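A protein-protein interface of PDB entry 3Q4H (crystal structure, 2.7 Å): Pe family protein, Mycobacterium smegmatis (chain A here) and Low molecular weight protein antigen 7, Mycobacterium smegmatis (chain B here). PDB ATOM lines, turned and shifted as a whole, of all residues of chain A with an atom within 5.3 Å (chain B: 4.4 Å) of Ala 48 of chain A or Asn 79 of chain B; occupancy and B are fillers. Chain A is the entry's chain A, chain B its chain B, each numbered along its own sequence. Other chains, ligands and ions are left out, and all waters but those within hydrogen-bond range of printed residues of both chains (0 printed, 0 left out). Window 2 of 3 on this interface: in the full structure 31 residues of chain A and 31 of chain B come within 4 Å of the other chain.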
ATOM      1  N   PHE A  43      27.365  12.683  25.477  1.00  0.00           N
ATOM      2  CA  PHE A  43      26.332  12.806  24.445  1.00  0.00           C
ATOM      3  C   PHE A  43      25.436  11.569  24.248  1.00  0.00           C
ATOM      4  O   PHE A  43      24.242  11.707  23.958  1.00  0.00           O
ATOM      5  CB  PHE A  43      26.990  13.182  23.111  1.00  0.00           C
ATOM      6  CG  PHE A  43      27.822  14.440  23.178  1.00  0.00           C
ATOM      7  CD1 PHE A  43      27.218  15.684  23.212  1.00  0.00           C
ATOM      8  CD2 PHE A  43      29.206  14.376  23.210  1.00  0.00           C
ATOM      9  CE1 PHE A  43      27.976  16.848  23.270  1.00  0.00           C
ATOM     10  CE2 PHE A  43      29.968  15.536  23.269  1.00  0.00           C
ATOM     11  CZ  PHE A  43      29.348  16.773  23.300  1.00  0.00           C
ATOM     12  N   HIS A  44      26.006  10.377  24.434  1.00  0.00           N
ATOM     13  CA  HIS A  44      25.350   9.115  24.053  1.00  0.00           C
ATOM     14  C   HIS A  44      24.435   8.553  25.142  1.00  0.00           C
ATOM     15  O   HIS A  44      24.354   9.110  26.237  1.00  0.00           O
ATOM     16  CB  HIS A  44      26.409   8.075  23.681  1.00  0.00           C
ATOM     17  CG  HIS A  44      27.495   8.622  22.813  1.00  0.00           C
ATOM     18  ND1 HIS A  44      27.256   9.106  21.547  1.00  0.00           N
ATOM     19  CD2 HIS A  44      28.817   8.797  23.041  1.00  0.00           C
ATOM     20  CE1 HIS A  44      28.387   9.542  21.023  1.00  0.00           C
ATOM     21  NE2 HIS A  44      29.350   9.365  21.909  1.00  0.00           N
ATOM     22  N   MET A  45      23.751   7.450  24.829  1.00  0.00           N
ATOM     23  CA  MET A  45      22.843   6.798  25.777  1.00  0.00           C
ATOM     24  C   MET A  45      22.558   5.338  25.396  1.00  0.00           C
ATOM     25  O   MET A  45      22.266   5.037  24.235  1.00  0.00           O
ATOM     26  CB  MET A  45      21.527   7.577  25.858  1.00  0.00           C
ATOM     27  N   GLY A  46      22.650   4.441  26.380  1.00  0.00           N
ATOM     28  CA  GLY A  46      22.277   3.033  26.201  1.00  0.00           C
ATOM     29  C   GLY A  46      23.239   2.213  25.351  1.00  0.00           C
ATOM     30  O   GLY A  46      24.354   1.903  25.780  1.00  0.00           O
ATOM     31  N   GLU A  47      22.795   1.863  24.142  1.00  0.00           N
ATOM     32  CA  GLU A  47      23.539   0.974  23.229  1.00  0.00           C
ATOM     33  C   GLU A  47      24.753   1.661  22.609  1.00  0.00           C
ATOM     34  O   GLU A  47      25.838   1.076  22.525  1.00  0.00           O
ATOM     35  CB  GLU A  47      22.608   0.453  22.116  1.00  0.00           C
ATOM     36  CG  GLU A  47      23.318  -0.174  20.906  1.00  0.00           C
ATOM     37  CD  GLU A  47      22.392  -1.016  20.029  1.00  0.00           C
ATOM     38  OE1 GLU A  47      21.169  -0.746  19.995  1.00  0.00           O
ATOM     39  OE2 GLU A  47      22.896  -1.955  19.370  1.00  0.00           O
ATOM     40  N   ALA A  48      24.556   2.894  22.149  1.00  0.00           N
ATOM     41  CA  ALA A  48      25.651   3.686  21.590  1.00  0.00           C
ATOM     42  C   ALA A  48      26.693   3.996  22.666  1.00  0.00           C
ATOM     43  O   ALA A  48      27.885   3.975  22.397  1.00  0.00           O
ATOM     44  CB  ALA A  48      25.114   4.973  20.981  1.00  0.00           C
ATOM     45  N   SER A  49      26.221   4.272  23.880  1.00  0.00           N
ATOM     46  CA  SER A  49      27.091   4.546  25.021  1.00  0.00           C
ATOM     47  C   SER A  49      27.895   3.316  25.432  1.00  0.00           C
ATOM     48  O   SER A  49      29.107   3.404  25.619  1.00  0.00           O
ATOM     49  CB  SER A  49      26.259   5.039  26.213  1.00  0.00           C
ATOM     50  OG  SER A  49      27.063   5.193  27.370  1.00  0.00           O
ATOM     51  N   ALA A  50      27.212   2.180  25.576  1.00  0.00           N
ATOM     52  CA  ALA A  50      27.845   0.928  25.999  1.00  0.00           C
ATOM     53  C   ALA A  50      28.985   0.545  25.063  1.00  0.00           C
ATOM     54  O   ALA A  50      30.058   0.161  25.516  1.00  0.00           O
ATOM     55  CB  ALA A  50      26.818  -0.184  26.065  1.00  0.00           C
ATOM     56  N   ALA A  51      28.738   0.666  23.760  1.00  0.00           N
ATOM     57  CA  ALA A  51      29.776   0.541  22.737  1.00  0.00           C
ATOM     58  C   ALA A  51      30.958   1.501  22.969  1.00  0.00           C
ATOM     59  O   ALA A  51      32.115   1.115  22.817  1.00  0.00           O
ATOM     60  CB  ALA A  51      29.179   0.773  21.357  1.00  0.00           C
ATOM     61  N   PHE A  52      30.661   2.748  23.327  1.00  0.00           N
ATOM     62  CA  PHE A  52      31.692   3.729  23.643  1.00  0.00           C
ATOM     63  C   PHE A  52      32.481   3.327  24.887  1.00  0.00           C
ATOM     64  O   PHE A  52      33.711   3.268  24.856  1.00  0.00           O
ATOM     65  CB  PHE A  52      31.071   5.111  23.855  1.00  0.00           C
ATOM     66  CG  PHE A  52      32.076   6.223  23.895  1.00  0.00           C
ATOM     67  CD1 PHE A  52      32.721   6.549  25.078  1.00  0.00           C
ATOM     68  CD2 PHE A  52      32.380   6.940  22.743  1.00  0.00           C
ATOM     69  CE1 PHE A  52      33.655   7.568  25.115  1.00  0.00           C
ATOM     70  CE2 PHE A  52      33.302   7.956  22.769  1.00  0.00           C
ATOM     71  CZ  PHE A  52      33.950   8.273  23.956  1.00  0.00           C
ATOM     72  N   MET B  11      28.886  17.961  18.984  1.00  0.00           N
ATOM     73  CA  MET B  11      29.204  16.559  18.784  1.00  0.00           C
ATOM     74  C   MET B  11      30.146  16.344  17.618  1.00  0.00           C
ATOM     75  O   MET B  11      31.127  15.624  17.750  1.00  0.00           O
ATOM     76  CB  MET B  11      27.923  15.756  18.584  1.00  0.00           C
ATOM     77  CG  MET B  11      27.103  15.685  19.852  1.00  0.00           C
ATOM     78  SD  MET B  11      25.533  14.545  19.717  1.00  0.00           S
ATOM     79  CE  MET B  11      26.433  12.801  19.640  1.00  0.00           C
ATOM     80  N   THR B  75      32.009   5.346  16.582  1.00  0.00           N
ATOM     81  CA  THR B  75      30.767   5.161  17.328  1.00  0.00           C
ATOM     82  C   THR B  75      30.172   6.511  17.675  1.00  0.00           C
ATOM     83  O   THR B  75      28.956   6.699  17.601  1.00  0.00           O
ATOM     84  CB  THR B  75      30.986   4.368  18.626  1.00  0.00           C
ATOM     85  OG1 THR B  75      31.813   3.233  18.353  1.00  0.00           O
ATOM     86  CG2 THR B  75      29.659   3.893  19.201  1.00  0.00           C
ATOM     87  N   HIS B  76      31.042   7.447  18.049  1.00  0.00           N
ATOM     88  CA  HIS B  76      30.623   8.816  18.300  1.00  0.00           C
ATOM     89  C   HIS B  76      30.092   9.462  17.016  1.00  0.00           C
ATOM     90  O   HIS B  76      29.043  10.107  17.040  1.00  0.00           O
ATOM     91  CB  HIS B  76      31.774   9.637  18.891  1.00  0.00           C
ATOM     92  CG  HIS B  76      31.405  11.056  19.190  1.00  0.00           C
ATOM     93  ND1 HIS B  76      30.735  11.426  20.334  1.00  0.00           N
ATOM     94  CD2 HIS B  76      31.588  12.193  18.477  1.00  0.00           C
ATOM     95  CE1 HIS B  76      30.528  12.729  20.318  1.00  0.00           C
ATOM     96  NE2 HIS B  76      31.038  13.220  19.204  1.00  0.00           N
ATOM     97  N   GLU B  77      30.815   9.267  15.909  1.00  0.00           N
ATOM     98  CA  GLU B  77      30.430   9.802  14.598  1.00  0.00           C
ATOM     99  C   GLU B  77      29.117   9.207  14.091  1.00  0.00           C
ATOM    100  O   GLU B  77      28.213   9.942  13.691  1.00  0.00           O
ATOM    101  CB  GLU B  77      31.532   9.543  13.568  1.00  0.00           C
ATOM    102  N   GLN B  78      29.020   7.880  14.107  1.00  0.00           N
ATOM    103  CA  GLN B  78      27.823   7.179  13.624  1.00  0.00           C
ATOM    104  C   GLN B  78      26.593   7.471  14.489  1.00  0.00           C
ATOM    105  O   GLN B  78      25.463   7.443  13.995  1.00  0.00           O
ATOM    106  CB  GLN B  78      28.066   5.666  13.554  1.00  0.00           C
ATOM    107  N   ASN B  79      26.814   7.756  15.771  1.00  0.00           N
ATOM    108  CA  ASN B  79      25.725   8.081  16.693  1.00  0.00           C
ATOM    109  C   ASN B  79      25.169   9.488  16.463  1.00  0.00           C
ATOM    110  O   ASN B  79      23.958   9.680  16.410  1.00  0.00           O
ATOM    111  CB  ASN B  79      26.206   7.936  18.136  1.00  0.00           C
ATOM    112  CG  ASN B  79      25.137   8.269  19.137  1.00  0.00           C
ATOM    113  OD1 ASN B  79      25.272   9.214  19.912  1.00  0.00           O
ATOM    114  ND2 ASN B  79      24.056   7.504  19.122  1.00  0.00           N
ATOM    115  N   THR B  80      26.069  10.459  16.332  1.00  0.00           N
ATOM    116  CA  THR B  80      25.706  11.860  16.088  1.00  0.00           C
ATOM    117  C   THR B  80      24.885  12.061  14.816  1.00  0.00           C
ATOM    118  O   THR B  80      23.938  12.844  14.806  1.00  0.00           O
ATOM    119  CB  THR B  80      26.959  12.734  15.950  1.00  0.00           C
ATOM    120  OG1 THR B  80      27.891  12.401  16.986  1.00  0.00           O
ATOM    121  CG2 THR B  80      26.596  14.204  16.040  1.00  0.00           C
ATOM    122  N   MET B  81      25.266  11.371  13.744  1.00  0.00           N
ATOM    123  CA  MET B  81      24.531  11.427  12.481  1.00  0.00           C
ATOM    124  C   MET B  81      23.084  10.973  12.675  1.00  0.00           C
ATOM    125  O   MET B  81      22.174  11.485  12.017  1.00  0.00           O
ATOM    126  CB  MET B  81      25.215  10.560  11.420  1.00  0.00           C
ATOM    127  N   ALA B  82      22.881  10.019  13.586  1.00  0.00           N
ATOM    128  CA  ALA B  82      21.542   9.553  13.961  1.00  0.00           C
ATOM    129  C   ALA B  82      20.752  10.600  14.764  1.00  0.00           C
ATOM    130  O   ALA B  82      19.516  10.630  14.709  1.00  0.00           O
ATOM    131  CB  ALA B  82      21.639   8.245  14.748  1.00  0.00           C
ATOM    132  N   MET B  83      21.466  11.453  15.504  1.00  0.00           N
ATOM    133  CA  MET B  83      20.834  12.501  16.316  1.00  0.00           C
ATOM    134  C   MET B  83      20.276  13.645  15.468  1.00  0.00           C
ATOM    135  O   MET B  83      19.163  14.110  15.721  1.00  0.00           O
ATOM    136  CB  MET B  83      21.818  13.064  17.353  1.00  0.00           C
ATOM    137  CG  MET B  83      22.398  12.026  18.320  1.00  0.00           C
ATOM    138  SD  MET B  83      21.050  10.898  19.200  1.00  0.00           S
ATOM    139  CE  MET B  83      22.230   9.855  20.366  1.00  0.00           C
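Among the printed residues, merely in contact across the chains: Ala 48 of chain A with Asn 79 of chain B (3.3 Å), Phe 43 of chain A with Met 11 of chain B (3.4 Å), Phe 43 of chain A with His 76 of chain B (3.6 Å), Ala 48 of chain A with Thr 75 of chain B (3.7 Å) and Ala 51 of chain A with Thr 75 of chain B (3.8 Å).
O of Met 11 of chain B lies within hydrogen-bond range of NE2 of His 76 of chain B (2.8 Å).
O of His 76 of chain B lies within hydrogen-bond range of OG1 of Thr 80 of chain B.
A ring nitrogen (ND1) of His 44 of chain A is in hydrogen-bond range of the side-chain amide oxygen (OD1) of Asn 79 of chain B (2.6 Å).
ND1 of His 76 of chain B sits at hydrogen-bond distance from NE2 of His 44 of chain A, 2.9 Å away.
Of the printed residues of chain B, Phe 43 of chain A touches Met 11 and His 76.
Of the printed residues of chain B, His 44 of chain A touches His 76 and Asn 79.
Ala 48 of chain A touches just these residues of chain B: Thr 75 (3.7 Å) and Asn 79 (3.3 Å).
Of the printed residues of chain A, Met 11 of chain B touches Phe 43.
Printed residues of chain A within 4 Å of Thr 75 of chain B: Ala 48 and Ala 51.
Printed residues of chain A within 4 Å of His 76 of chain B: Phe 43 and His 44.
Glu 77 of chain B touches none of the printed residues of chain A.
Met 81 of chain B touches none of the printed residues of chain A.
The nearest printed residue of chain B that does not touch Ala 48 of chain A is Met 83 of chain B (5.7 Å).
Of the 10 printed residues of chain A, 4 touch a printed residue of chain B.
Of the 10 printed residues of chain B, 4 touch a printed residue of chain A.
Hydrophobic or aromatic side chains of chain B that line the printed part of chain A: Met 11 and His 76.
Among the printed residues, 7 pairs touch across the chains.
Among the printed residues, no Asp or Glu carboxylate lies within 4 Å of a Lys or Arg side-chain nitrogen of the other chain.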
